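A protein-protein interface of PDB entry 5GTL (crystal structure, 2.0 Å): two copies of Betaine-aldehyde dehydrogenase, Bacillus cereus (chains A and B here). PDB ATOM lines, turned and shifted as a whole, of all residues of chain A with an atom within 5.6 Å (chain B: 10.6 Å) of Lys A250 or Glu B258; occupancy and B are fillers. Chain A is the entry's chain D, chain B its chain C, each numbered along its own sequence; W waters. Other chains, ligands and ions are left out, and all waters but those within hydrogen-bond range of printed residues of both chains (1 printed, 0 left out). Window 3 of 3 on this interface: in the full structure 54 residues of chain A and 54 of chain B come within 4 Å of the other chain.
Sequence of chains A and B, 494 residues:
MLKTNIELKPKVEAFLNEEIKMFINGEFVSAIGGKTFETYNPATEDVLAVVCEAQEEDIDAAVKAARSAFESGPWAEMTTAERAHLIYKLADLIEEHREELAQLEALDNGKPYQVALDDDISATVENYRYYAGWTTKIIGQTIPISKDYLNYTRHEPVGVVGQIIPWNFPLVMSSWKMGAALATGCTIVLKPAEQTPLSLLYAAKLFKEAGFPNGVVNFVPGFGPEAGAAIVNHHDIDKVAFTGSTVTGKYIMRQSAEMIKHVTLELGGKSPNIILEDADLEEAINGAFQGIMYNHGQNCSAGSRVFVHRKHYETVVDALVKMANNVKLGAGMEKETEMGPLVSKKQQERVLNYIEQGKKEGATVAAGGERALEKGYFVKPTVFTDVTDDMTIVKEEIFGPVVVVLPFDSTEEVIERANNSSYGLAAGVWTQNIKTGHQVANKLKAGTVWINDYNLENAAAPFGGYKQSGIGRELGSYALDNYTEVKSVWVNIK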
ATOM      1  N   SER A 245       2.317 -19.187 -31.912  1.00  0.00           N
ATOM      2  CA  SER A 245       1.842 -17.858 -32.224  1.00  0.00           C
ATOM      3  C   SER A 245       1.587 -17.079 -30.965  1.00  0.00           C
ATOM      4  O   SER A 245       1.192 -17.631 -29.887  1.00  0.00           O
ATOM      5  CB  SER A 245       0.508 -17.895 -33.010  1.00  0.00           C
ATOM      6  OG  SER A 245      -0.469 -18.640 -32.313  1.00  0.00           O
ATOM      7  N   THR A 246       1.745 -15.767 -31.122  1.00  0.00           N
ATOM      8  CA  THR A 246       1.460 -14.852 -30.050  1.00  0.00           C
ATOM      9  C   THR A 246       0.011 -15.083 -29.551  1.00  0.00           C
ATOM     10  O   THR A 246      -0.254 -15.092 -28.334  1.00  0.00           O
ATOM     11  CB  THR A 246       1.821 -13.403 -30.509  1.00  0.00           C
ATOM     12  OG1 THR A 246       3.256 -13.316 -30.613  1.00  0.00           O
ATOM     13  CG2 THR A 246       1.325 -12.343 -29.510  1.00  0.00           C
ATOM     14  N   VAL A 247      -0.916 -15.312 -30.480  1.00  0.00           N
ATOM     15  CA  VAL A 247      -2.346 -15.445 -30.135  1.00  0.00           C
ATOM     16  C   VAL A 247      -2.649 -16.667 -29.237  1.00  0.00           C
ATOM     17  O   VAL A 247      -3.299 -16.555 -28.189  1.00  0.00           O
ATOM     18  CB  VAL A 247      -3.234 -15.367 -31.425  1.00  0.00           C
ATOM     19  CG1 VAL A 247      -3.085 -16.613 -32.309  1.00  0.00           C
ATOM     20  CG2 VAL A 247      -4.694 -15.136 -31.069  1.00  0.00           C
ATOM     21  N   THR A 248      -2.101 -17.826 -29.595  1.00  0.00           N
ATOM     22  CA  THR A 248      -2.250 -19.037 -28.772  1.00  0.00           C
ATOM     23  C   THR A 248      -1.488 -18.900 -27.455  1.00  0.00           C
ATOM     24  O   THR A 248      -1.933 -19.406 -26.388  1.00  0.00           O
ATOM     25  CB  THR A 248      -1.742 -20.269 -29.537  1.00  0.00           C
ATOM     26  OG1 THR A 248      -2.152 -20.164 -30.892  1.00  0.00           O
ATOM     27  CG2 THR A 248      -2.294 -21.563 -28.963  1.00  0.00           C
ATOM     28  N   GLY A 249      -0.357 -18.192 -27.510  1.00  0.00           N
ATOM     29  CA  GLY A 249       0.385 -17.856 -26.283  1.00  0.00           C
ATOM     30  C   GLY A 249      -0.444 -17.149 -25.227  1.00  0.00           C
ATOM     31  O   GLY A 249      -0.421 -17.514 -24.017  1.00  0.00           O
ATOM     32  N   LYS A 250      -1.221 -16.151 -25.700  1.00  0.00           N
ATOM     33  CA  LYS A 250      -2.182 -15.424 -24.829  1.00  0.00           C
ATOM     34  C   LYS A 250      -3.094 -16.403 -24.155  1.00  0.00           C
ATOM     35  O   LYS A 250      -3.253 -16.376 -22.891  1.00  0.00           O
ATOM     36  CB  LYS A 250      -2.991 -14.402 -25.640  1.00  0.00           C
ATOM     37  CG  LYS A 250      -2.127 -13.265 -26.133  1.00  0.00           C
ATOM     38  CD  LYS A 250      -2.680 -12.449 -27.304  1.00  0.00           C
ATOM     39  CE  LYS A 250      -2.187 -11.007 -27.192  1.00  0.00           C
ATOM     40  NZ  LYS A 250      -1.870 -10.240 -28.416  1.00  0.00           N
ATOM     41  N   TYR A 251      -3.670 -17.288 -24.998  1.00  0.00           N
ATOM     42  CA  TYR A 251      -4.580 -18.376 -24.563  1.00  0.00           C
ATOM     43  C   TYR A 251      -3.968 -19.215 -23.432  1.00  0.00           C
ATOM     44  O   TYR A 251      -4.524 -19.288 -22.286  1.00  0.00           O
ATOM     45  CB  TYR A 251      -5.037 -19.261 -25.765  1.00  0.00           C
ATOM     46  CG  TYR A 251      -5.761 -20.524 -25.326  1.00  0.00           C
ATOM     47  CD1 TYR A 251      -7.084 -20.484 -24.898  1.00  0.00           C
ATOM     48  CD2 TYR A 251      -5.099 -21.755 -25.288  1.00  0.00           C
ATOM     49  CE1 TYR A 251      -7.733 -21.628 -24.459  1.00  0.00           C
ATOM     50  CE2 TYR A 251      -5.748 -22.909 -24.848  1.00  0.00           C
ATOM     51  CZ  TYR A 251      -7.067 -22.838 -24.442  1.00  0.00           C
ATOM     52  OH  TYR A 251      -7.702 -23.979 -24.003  1.00  0.00           O
ATOM     53  N   ILE A 252      -2.772 -19.749 -23.711  1.00  0.00           N
ATOM     54  CA  ILE A 252      -2.022 -20.554 -22.731  1.00  0.00           C
ATOM     55  C   ILE A 252      -1.815 -19.830 -21.385  1.00  0.00           C
ATOM     56  O   ILE A 252      -2.099 -20.367 -20.287  1.00  0.00           O
ATOM     57  CB  ILE A 252      -0.729 -21.096 -23.397  1.00  0.00           C
ATOM     58  CG1 ILE A 252      -1.122 -22.307 -24.270  1.00  0.00           C
ATOM     59  CG2 ILE A 252       0.291 -21.578 -22.388  1.00  0.00           C
ATOM     60  CD1 ILE A 252      -0.477 -22.294 -25.609  1.00  0.00           C
ATOM     61  N   MET A 253      -1.403 -18.571 -21.457  1.00  0.00           N
ATOM     62  CA  MET A 253      -1.174 -17.822 -20.218  1.00  0.00           C
ATOM     63  C   MET A 253      -2.455 -17.554 -19.482  1.00  0.00           C
ATOM     64  O   MET A 253      -2.512 -17.713 -18.234  1.00  0.00           O
ATOM     65  CB  MET A 253      -0.454 -16.506 -20.504  1.00  0.00           C
ATOM     66  CG  MET A 253       0.396 -16.087 -19.339  1.00  0.00           C
ATOM     67  SD  MET A 253       1.300 -14.582 -19.685  1.00  0.00           S
ATOM     68  CE  MET A 253       1.276 -13.991 -17.988  1.00  0.00           C
ATOM     69  N   ARG A 254      -3.497 -17.181 -20.260  1.00  0.00           N
ATOM     70  CA  ARG A 254      -4.837 -17.023 -19.698  1.00  0.00           C
ATOM     71  C   ARG A 254      -5.266 -18.280 -18.988  1.00  0.00           C
ATOM     72  O   ARG A 254      -5.695 -18.223 -17.840  1.00  0.00           O
ATOM     73  CB  ARG A 254      -5.859 -16.640 -20.760  1.00  0.00           C
ATOM     74  CG  ARG A 254      -7.090 -15.951 -20.213  1.00  0.00           C
ATOM     75  CD  ARG A 254      -8.056 -15.617 -21.327  1.00  0.00           C
ATOM     76  NE  ARG A 254      -7.363 -15.079 -22.525  1.00  0.00           N
ATOM     77  CZ  ARG A 254      -7.295 -15.661 -23.743  1.00  0.00           C
ATOM     78  NH1 ARG A 254      -7.882 -16.852 -23.998  1.00  0.00           N
ATOM     79  NH2 ARG A 254      -6.629 -15.049 -24.736  1.00  0.00           N
ATOM     80  N   GLN A 255      -5.132 -19.423 -19.655  1.00  0.00           N
ATOM     81  CA  GLN A 255      -5.541 -20.686 -19.028  1.00  0.00           C
ATOM     82  C   GLN A 255      -4.679 -21.038 -17.836  1.00  0.00           C
ATOM     83  O   GLN A 255      -5.165 -21.613 -16.832  1.00  0.00           O
ATOM     84  CB  GLN A 255      -5.511 -21.852 -20.035  1.00  0.00           C
ATOM     85  CG  GLN A 255      -6.430 -21.720 -21.252  1.00  0.00           C
ATOM     86  CD  GLN A 255      -7.841 -21.336 -20.857  1.00  0.00           C
ATOM     87  OE1 GLN A 255      -8.335 -20.269 -21.226  1.00  0.00           O
ATOM     88  NE2 GLN A 255      -8.458 -22.168 -20.034  1.00  0.00           N
ATOM     89  N   LEU A 267       7.146 -16.916 -28.677  1.00  0.00           N
ATOM     90  CA  LEU A 267       6.156 -16.578 -29.634  1.00  0.00           C
ATOM     91  C   LEU A 267       6.831 -16.084 -30.922  1.00  0.00           C
ATOM     92  O   LEU A 267       7.974 -16.376 -31.094  1.00  0.00           O
ATOM     93  CB  LEU A 267       5.180 -15.660 -28.966  1.00  0.00           C
ATOM     94  CG  LEU A 267       4.754 -16.194 -27.584  1.00  0.00           C
ATOM     95  CD1 LEU A 267       4.047 -15.252 -26.653  1.00  0.00           C
ATOM     96  CD2 LEU A 267       4.076 -17.540 -27.554  1.00  0.00           C
ATOM     97  N   GLN A 468       5.997  -8.841 -26.900  1.00  0.00           N
ATOM     98  CA  GLN A 468       5.057  -9.943 -27.168  1.00  0.00           C
ATOM     99  C   GLN A 468       5.685 -11.092 -27.975  1.00  0.00           C
ATOM    100  O   GLN A 468       4.971 -11.927 -28.536  1.00  0.00           O
ATOM    101  CB  GLN A 468       3.757  -9.422 -27.812  1.00  0.00           C
ATOM    102  CG  GLN A 468       3.030  -8.488 -26.869  1.00  0.00           C
ATOM    103  CD  GLN A 468       1.678  -8.032 -27.381  1.00  0.00           C
ATOM    104  OE1 GLN A 468       0.941  -8.769 -28.052  1.00  0.00           O
ATOM    105  NE2 GLN A 468       1.329  -6.813 -27.032  1.00  0.00           N
ATOM    106  N   VAL B 232      -2.514  -2.821 -13.969  1.00  0.00           N
ATOM    107  CA  VAL B 232      -2.502  -4.155 -14.607  1.00  0.00           C
ATOM    108  C   VAL B 232      -2.799  -4.149 -16.146  1.00  0.00           C
ATOM    109  O   VAL B 232      -2.115  -4.828 -16.922  1.00  0.00           O
ATOM    110  CB  VAL B 232      -3.398  -5.157 -13.820  1.00  0.00           C
ATOM    111  CG1 VAL B 232      -4.854  -5.017 -14.192  1.00  0.00           C
ATOM    112  CG2 VAL B 232      -2.990  -6.584 -14.119  1.00  0.00           C
ATOM    113  N   ASN B 233      -3.771  -3.336 -16.579  1.00  0.00           N
ATOM    114  CA  ASN B 233      -4.212  -3.268 -17.981  1.00  0.00           C
ATOM    115  C   ASN B 233      -3.456  -2.286 -18.822  1.00  0.00           C
ATOM    116  O   ASN B 233      -3.669  -2.234 -20.035  1.00  0.00           O
ATOM    117  CB  ASN B 233      -5.724  -2.940 -18.062  1.00  0.00           C
ATOM    118  CG  ASN B 233      -6.582  -3.976 -17.338  1.00  0.00           C
ATOM    119  OD1 ASN B 233      -6.378  -5.182 -17.486  1.00  0.00           O
ATOM    120  ND2 ASN B 233      -7.500  -3.513 -16.499  1.00  0.00           N
ATOM    121  N   HIS B 234      -2.526  -1.530 -18.226  1.00  0.00           N
ATOM    122  CA  HIS B 234      -1.837  -0.477 -18.966  1.00  0.00           C
ATOM    123  C   HIS B 234      -0.881  -1.011 -20.072  1.00  0.00           C
ATOM    124  O   HIS B 234       0.019  -1.821 -19.789  1.00  0.00           O
ATOM    125  CB  HIS B 234      -1.086   0.459 -17.983  1.00  0.00           C
ATOM    126  CG  HIS B 234      -0.841   1.790 -18.571  1.00  0.00           C
ATOM    127  ND1 HIS B 234      -0.009   1.941 -19.652  1.00  0.00           N
ATOM    128  CD2 HIS B 234      -1.465   2.982 -18.403  1.00  0.00           C
ATOM    129  CE1 HIS B 234      -0.046   3.196 -20.071  1.00  0.00           C
ATOM    130  NE2 HIS B 234      -0.932   3.844 -19.336  1.00  0.00           N
ATOM    131  N   HIS B 235      -1.062  -0.549 -21.298  1.00  0.00           N
ATOM    132  CA  HIS B 235      -0.267  -0.953 -22.449  1.00  0.00           C
ATOM    133  C   HIS B 235       1.226  -0.634 -22.461  1.00  0.00           C
ATOM    134  O   HIS B 235       1.967  -1.260 -23.174  1.00  0.00           O
ATOM    135  CB  HIS B 235      -0.855  -0.389 -23.740  1.00  0.00           C
ATOM    136  CG  HIS B 235      -0.505   1.047 -23.982  1.00  0.00           C
ATOM    137  ND1 HIS B 235      -1.066   2.075 -23.272  1.00  0.00           N
ATOM    138  CD2 HIS B 235       0.358   1.620 -24.847  1.00  0.00           C
ATOM    139  CE1 HIS B 235      -0.562   3.217 -23.684  1.00  0.00           C
ATOM    140  NE2 HIS B 235       0.310   2.969 -24.638  1.00  0.00           N
ATOM    141  N   ILE B 237       3.184  -0.599 -19.640  1.00  0.00           N
ATOM    142  CA  ILE B 237       3.825  -1.129 -18.478  1.00  0.00           C
ATOM    143  C   ILE B 237       4.407  -2.462 -18.917  1.00  0.00           C
ATOM    144  O   ILE B 237       3.726  -3.301 -19.409  1.00  0.00           O
ATOM    145  CB  ILE B 237       2.909  -1.265 -17.268  1.00  0.00           C
ATOM    146  CG1 ILE B 237       2.738   0.074 -16.582  1.00  0.00           C
ATOM    147  CG2 ILE B 237       3.516  -2.185 -16.233  1.00  0.00           C
ATOM    148  CD1 ILE B 237       1.708   0.062 -15.505  1.00  0.00           C
ATOM    149  N   ASP B 238       5.698  -2.597 -18.730  1.00  0.00           N
ATOM    150  CA  ASP B 238       6.429  -3.767 -19.147  1.00  0.00           C
ATOM    151  C   ASP B 238       6.298  -5.026 -18.325  1.00  0.00           C
ATOM    152  O   ASP B 238       6.387  -6.088 -18.860  1.00  0.00           O
ATOM    153  CB  ASP B 238       7.895  -3.415 -19.334  1.00  0.00           C
ATOM    154  CG  ASP B 238       8.118  -2.352 -20.379  1.00  0.00           C
ATOM    155  OD1 ASP B 238       7.802  -2.574 -21.506  1.00  0.00           O
ATOM    156  OD2 ASP B 238       8.624  -1.301 -20.086  1.00  0.00           O
ATOM    157  N   VAL B 240       4.606  -6.691 -14.360  1.00  0.00           N
ATOM    158  CA  VAL B 240       3.813  -6.449 -13.183  1.00  0.00           C
ATOM    159  C   VAL B 240       4.154  -7.382 -12.060  1.00  0.00           C
ATOM    160  O   VAL B 240       4.490  -8.482 -12.282  1.00  0.00           O
ATOM    161  CB  VAL B 240       2.282  -6.582 -13.513  1.00  0.00           C
ATOM    162  CG1 VAL B 240       1.899  -8.030 -13.664  1.00  0.00           C
ATOM    163  CG2 VAL B 240       1.403  -5.971 -12.459  1.00  0.00           C
ATOM    164  N   LYS B 250      -5.158 -14.520  -9.809  1.00  0.00           N
ATOM    165  CA  LYS B 250      -5.647 -15.157 -11.045  1.00  0.00           C
ATOM    166  C   LYS B 250      -6.026 -14.111 -12.059  1.00  0.00           C
ATOM    167  O   LYS B 250      -5.597 -14.176 -13.229  1.00  0.00           O
ATOM    168  CB  LYS B 250      -6.850 -16.067 -10.780  1.00  0.00           C
ATOM    169  CG  LYS B 250      -6.518 -17.295  -9.970  1.00  0.00           C
ATOM    170  CD  LYS B 250      -7.666 -18.295  -9.901  1.00  0.00           C
ATOM    171  CE  LYS B 250      -7.288 -19.418  -8.942  1.00  0.00           C
ATOM    172  NZ  LYS B 250      -8.306 -20.496  -8.820  1.00  0.00           N
ATOM    173  N   TYR B 251      -6.816 -13.134 -11.588  1.00  0.00           N
ATOM    174  CA  TYR B 251      -7.170 -11.955 -12.379  1.00  0.00           C
ATOM    175  C   TYR B 251      -5.938 -11.248 -13.002  1.00  0.00           C
ATOM    176  O   TYR B 251      -5.862 -11.104 -14.259  1.00  0.00           O
ATOM    177  CB  TYR B 251      -8.064 -10.976 -11.541  1.00  0.00           C
ATOM    178  CG  TYR B 251      -8.212  -9.613 -12.173  1.00  0.00           C
ATOM    179  CD1 TYR B 251      -9.190  -9.361 -13.139  1.00  0.00           C
ATOM    180  CD2 TYR B 251      -7.345  -8.587 -11.836  1.00  0.00           C
ATOM    181  CE1 TYR B 251      -9.285  -8.120 -13.759  1.00  0.00           C
ATOM    182  CE2 TYR B 251      -7.440  -7.345 -12.444  1.00  0.00           C
ATOM    183  CZ  TYR B 251      -8.407  -7.114 -13.391  1.00  0.00           C
ATOM    184  OH  TYR B 251      -8.455  -5.871 -13.939  1.00  0.00           O
ATOM    185  N   ILE B 252      -4.957 -10.845 -12.173  1.00  0.00           N
ATOM    186  CA  ILE B 252      -3.773 -10.134 -12.741  1.00  0.00           C
ATOM    187  C   ILE B 252      -3.113 -10.953 -13.842  1.00  0.00           C
ATOM    188  O   ILE B 252      -2.765 -10.445 -14.916  1.00  0.00           O
ATOM    189  CB  ILE B 252      -2.746  -9.721 -11.653  1.00  0.00           C
ATOM    190  CG1 ILE B 252      -3.182  -8.382 -11.001  1.00  0.00           C
ATOM    191  CG2 ILE B 252      -1.357  -9.514 -12.224  1.00  0.00           C
ATOM    192  CD1 ILE B 252      -3.782  -8.558  -9.638  1.00  0.00           C
ATOM    193  N   MET B 253      -2.979 -12.247 -13.597  1.00  0.00           N
ATOM    194  CA  MET B 253      -2.333 -13.109 -14.599  1.00  0.00           C
ATOM    195  C   MET B 253      -3.112 -13.186 -15.905  1.00  0.00           C
ATOM    196  O   MET B 253      -2.555 -13.048 -17.057  1.00  0.00           O
ATOM    197  CB  MET B 253      -2.108 -14.500 -14.014  1.00  0.00           C
ATOM    198  CG  MET B 253      -1.040 -15.242 -14.752  1.00  0.00           C
ATOM    199  SD  MET B 253      -0.473 -16.695 -13.910  1.00  0.00           S
ATOM    200  CE  MET B 253       0.325 -17.353 -15.392  1.00  0.00           C
ATOM    201  N   ARG B 254      -4.426 -13.380 -15.721  1.00  0.00           N
ATOM    202  CA  ARG B 254      -5.346 -13.393 -16.832  1.00  0.00           C
ATOM    203  C   ARG B 254      -5.195 -12.137 -17.644  1.00  0.00           C
ATOM    204  O   ARG B 254      -4.999 -12.232 -18.861  1.00  0.00           O
ATOM    205  CB  ARG B 254      -6.780 -13.574 -16.334  1.00  0.00           C
ATOM    206  CG  ARG B 254      -7.770 -14.063 -17.374  1.00  0.00           C
ATOM    207  CD  ARG B 254      -9.175 -14.066 -16.800  1.00  0.00           C
ATOM    208  NE  ARG B 254      -9.200 -14.766 -15.503  1.00  0.00           N
ATOM    209  CZ  ARG B 254      -9.615 -14.270 -14.326  1.00  0.00           C
ATOM    210  NH1 ARG B 254     -10.094 -13.029 -14.194  1.00  0.00           N
ATOM    211  NH2 ARG B 254      -9.571 -15.045 -13.245  1.00  0.00           N
ATOM    212  N   GLN B 255      -5.216 -10.968 -16.978  1.00  0.00           N
ATOM    213  CA  GLN B 255      -5.072  -9.694 -17.687  1.00  0.00           C
ATOM    214  C   GLN B 255      -3.699  -9.523 -18.302  1.00  0.00           C
ATOM    215  O   GLN B 255      -3.567  -8.935 -19.394  1.00  0.00           O
ATOM    216  CB  GLN B 255      -5.337  -8.475 -16.771  1.00  0.00           C
ATOM    217  CG  GLN B 255      -6.694  -8.403 -16.101  1.00  0.00           C
ATOM    218  CD  GLN B 255      -7.804  -8.567 -17.099  1.00  0.00           C
ATOM    219  OE1 GLN B 255      -8.429  -9.627 -17.172  1.00  0.00           O
ATOM    220  NE2 GLN B 255      -8.008  -7.549 -17.923  1.00  0.00           N
ATOM    221  N   SER B 256      -2.675 -10.017 -17.603  1.00  0.00           N
ATOM    222  CA  SER B 256      -1.306  -9.852 -18.082  1.00  0.00           C
ATOM    223  C   SER B 256      -1.064 -10.650 -19.367  1.00  0.00           C
ATOM    224  O   SER B 256      -0.336 -10.186 -20.264  1.00  0.00           O
ATOM    225  CB  SER B 256      -0.316 -10.194 -17.000  1.00  0.00           C
ATOM    226  OG  SER B 256      -0.487  -9.357 -15.864  1.00  0.00           O
ATOM    227  N   ALA B 257      -1.742 -11.811 -19.471  1.00  0.00           N
ATOM    228  CA  ALA B 257      -1.727 -12.647 -20.673  1.00  0.00           C
ATOM    229  C   ALA B 257      -1.983 -11.869 -21.923  1.00  0.00           C
ATOM    230  O   ALA B 257      -1.393 -12.149 -22.964  1.00  0.00           O
ATOM    231  CB  ALA B 257      -2.776 -13.744 -20.576  1.00  0.00           C
ATOM    232  N   GLU B 258      -2.881 -10.893 -21.848  1.00  0.00           N
ATOM    233  CA  GLU B 258      -3.248 -10.142 -23.037  1.00  0.00           C
ATOM    234  C   GLU B 258      -2.070  -9.439 -23.736  1.00  0.00           C
ATOM    235  O   GLU B 258      -2.093  -9.261 -24.956  1.00  0.00           O
ATOM    236  CB  GLU B 258      -4.380  -9.145 -22.696  1.00  0.00           C
ATOM    237  CG  GLU B 258      -5.117  -8.558 -23.899  1.00  0.00           C
ATOM    238  CD  GLU B 258      -5.566  -9.607 -24.917  1.00  0.00           C
ATOM    239  OE1 GLU B 258      -5.414  -9.341 -26.140  1.00  0.00           O
ATOM    240  OE2 GLU B 258      -6.030 -10.697 -24.487  1.00  0.00           O
ATOM    241  N   MET B 259      -1.056  -9.095 -22.966  1.00  0.00           N
ATOM    242  CA  MET B 259       0.121  -8.425 -23.457  1.00  0.00           C
ATOM    243  C   MET B 259       1.443  -9.202 -23.297  1.00  0.00           C
ATOM    244  O   MET B 259       2.491  -8.654 -23.438  1.00  0.00           O
ATOM    245  CB  MET B 259       0.234  -7.104 -22.737  1.00  0.00           C
ATOM    246  CG  MET B 259      -0.933  -6.179 -23.000  1.00  0.00           C
ATOM    247  SD  MET B 259      -0.989  -4.769 -21.916  1.00  0.00           S
ATOM    248  CE  MET B 259      -1.490  -5.411 -20.334  1.00  0.00           C
ATOM    249  N   ILE B 260       1.367 -10.485 -23.026  1.00  0.00           N
ATOM    250  CA  ILE B 260       2.542 -11.321 -22.846  1.00  0.00           C
ATOM    251  C   ILE B 260       3.517 -10.627 -21.899  1.00  0.00           C
ATOM    252  O   ILE B 260       4.657 -10.412 -22.205  1.00  0.00           O
ATOM    253  CB  ILE B 260       3.218 -11.670 -24.169  1.00  0.00           C
ATOM    254  CG1 ILE B 260       2.196 -12.143 -25.193  1.00  0.00           C
ATOM    255  CG2 ILE B 260       4.267 -12.731 -23.939  1.00  0.00           C
ATOM    256  CD1 ILE B 260       1.460 -13.368 -24.793  1.00  0.00           C
ATOM    257  N   LYS B 261       2.980 -10.290 -20.743  1.00  0.00           N
ATOM    258  CA  LYS B 261       3.635  -9.563 -19.700  1.00  0.00           C
ATOM    259  C   LYS B 261       4.008 -10.432 -18.520  1.00  0.00           C
ATOM    260  O   LYS B 261       3.167 -11.045 -17.954  1.00  0.00           O
ATOM    261  CB  LYS B 261       2.704  -8.449 -19.249  1.00  0.00           C
ATOM    262  CG  LYS B 261       3.339  -7.400 -18.390  1.00  0.00           C
ATOM    263  CD  LYS B 261       2.347  -6.338 -17.966  1.00  0.00           C
ATOM    264  CE  LYS B 261       1.484  -5.872 -19.110  1.00  0.00           C
ATOM    265  NZ  LYS B 261       0.998  -4.489 -18.982  1.00  0.00           N
ATOM    266  N   HIS B 262       5.284 -10.436 -18.179  1.00  0.00           N
ATOM    267  CA  HIS B 262       5.854 -11.171 -17.084  1.00  0.00           C
ATOM    268  C   HIS B 262       5.182 -10.820 -15.778  1.00  0.00           C
ATOM    269  O   HIS B 262       4.956  -9.699 -15.491  1.00  0.00           O
ATOM    270  CB  HIS B 262       7.338 -10.813 -16.987  1.00  0.00           C
ATOM    271  CG  HIS B 262       8.090 -11.560 -15.938  1.00  0.00           C
ATOM    272  ND1 HIS B 262       9.062 -12.475 -16.243  1.00  0.00           N
ATOM    273  CD2 HIS B 262       8.032 -11.511 -14.593  1.00  0.00           C
ATOM    274  CE1 HIS B 262       9.540 -12.987 -15.135  1.00  0.00           C
ATOM    275  NE2 HIS B 262       8.956 -12.397 -14.121  1.00  0.00           N
ATOM    276  N   VAL B 263       4.896 -11.810 -14.988  1.00  0.00           N
ATOM    277  CA  VAL B 263       4.246 -11.619 -13.734  1.00  0.00           C
ATOM    278  C   VAL B 263       4.948 -12.261 -12.576  1.00  0.00           C
ATOM    279  O   VAL B 263       5.492 -13.316 -12.704  1.00  0.00           O
ATOM    280  CB  VAL B 263       2.835 -12.246 -13.817  1.00  0.00           C
ATOM    281  CG1 VAL B 263       2.101 -12.079 -12.539  1.00  0.00           C
ATOM    282  CG2 VAL B 263       2.057 -11.591 -14.913  1.00  0.00           C
HETATM  283  O   HOH W   1      -6.154 -12.349 -22.247  1.00  0.00           O
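Among the printed residues, pairs that only touch across the chains: Lys A250 with Glu B258 (2.8 Å), Lys A250 with Ala B257 (3.4 Å), Arg A254 with Arg B254 (3.5 Å), Gln A468 with Met B259 (3.5 Å), Met A253 with Lys B261 (3.5 Å), Arg A254 with Ala B257 (3.5 Å), Met A253 with Ala B257 (3.6 Å), Leu A267 with Ile B260 (3.7 Å), Lys A250 with Ile B260 (3.8 Å), Gln A468 with Ile B260 (3.9 Å) and Met A253 with Val B263 (3.98 Å).
Water W1 lies within hydrogen-bond range of OE2 of Glu B258 (2.8 Å) and NE of Arg A254 (3.0 Å).
Arg B254 touches its own counterpart, Arg A254. Positions printed for both chains: 250, 251, 252, 253, 254 and 255. Of the 11 pairs that touch across the chains among the printed residues, 1 has its exchanged pair printed and touching as well.
The backbone carbonyl oxygen (O) of His B234 lies within hydrogen-bond range of the side-chain amino group (NZ) of Lys B261. The backbone carbonyl oxygen of Ile B237 is in hydrogen-bond range of the side-chain amino group of Lys B261 (3.0 Å). The backbone NH (N) of Lys B261 is in hydrogen-bond range of the backbone carbonyl oxygen (O) of Ser B256, 3.4 Å away. The side-chain amino group (NZ) of Lys B261 lies close to the side-chain sulfur (SD) of Met B259 (3.6 Å). OG1 of Thr A246 is in hydrogen-bond range of O of Gln A468 (3.0 Å). The side-chain amino group (NZ) of Lys A250 lies within hydrogen-bond range of the side-chain amide oxygen (OE1) of Gln A468.
No residue of chain B comes within 4 Å of Thr A246. No residue of chain B comes within 4 Å of Gly A249. Ile A252 touches none of the printed residues of chain B. Of chain B, only Ala B257, Lys B261 and Val B263 come within 4 Å of Met A253. Of the printed residues of chain B, Gln A468 touches Met B259 and Ile B260. Of the printed residues of chain A, Arg B254 touches Arg A254. Glu B258 touches just one residue of chain A: Lys A250 (2.8 Å). Of the printed residues of chain A, Met B259 touches Gln A468 (3.5 Å). Printed residues of chain A within 4 Å of Ile B260: Lys A250, Leu A267 and Gln A468. Printed residues of chain A within 4 Å of Val B263: Met A253 (3.98 Å). The nearest residue of chain B that does not touch Lys A250 is Met B259 (4.8 Å). The nearest printed residue of chain A that does not touch Ala B257 is Gly A249 (5.6 Å).
Hydrophobic or aromatic side chains of chain B that line the printed part of chain A: Ala B257, Ile B260 and Val B263. Hydrophobic or aromatic side chains of chain A that line the printed part of chain B: Met A253 and Leu A267. Among the printed residues, 11 pairs touch across the chains. Among the printed residues, no Asp or Glu carboxylate lies within 4 Å of a Lys or Arg side-chain nitrogen of the other chain.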
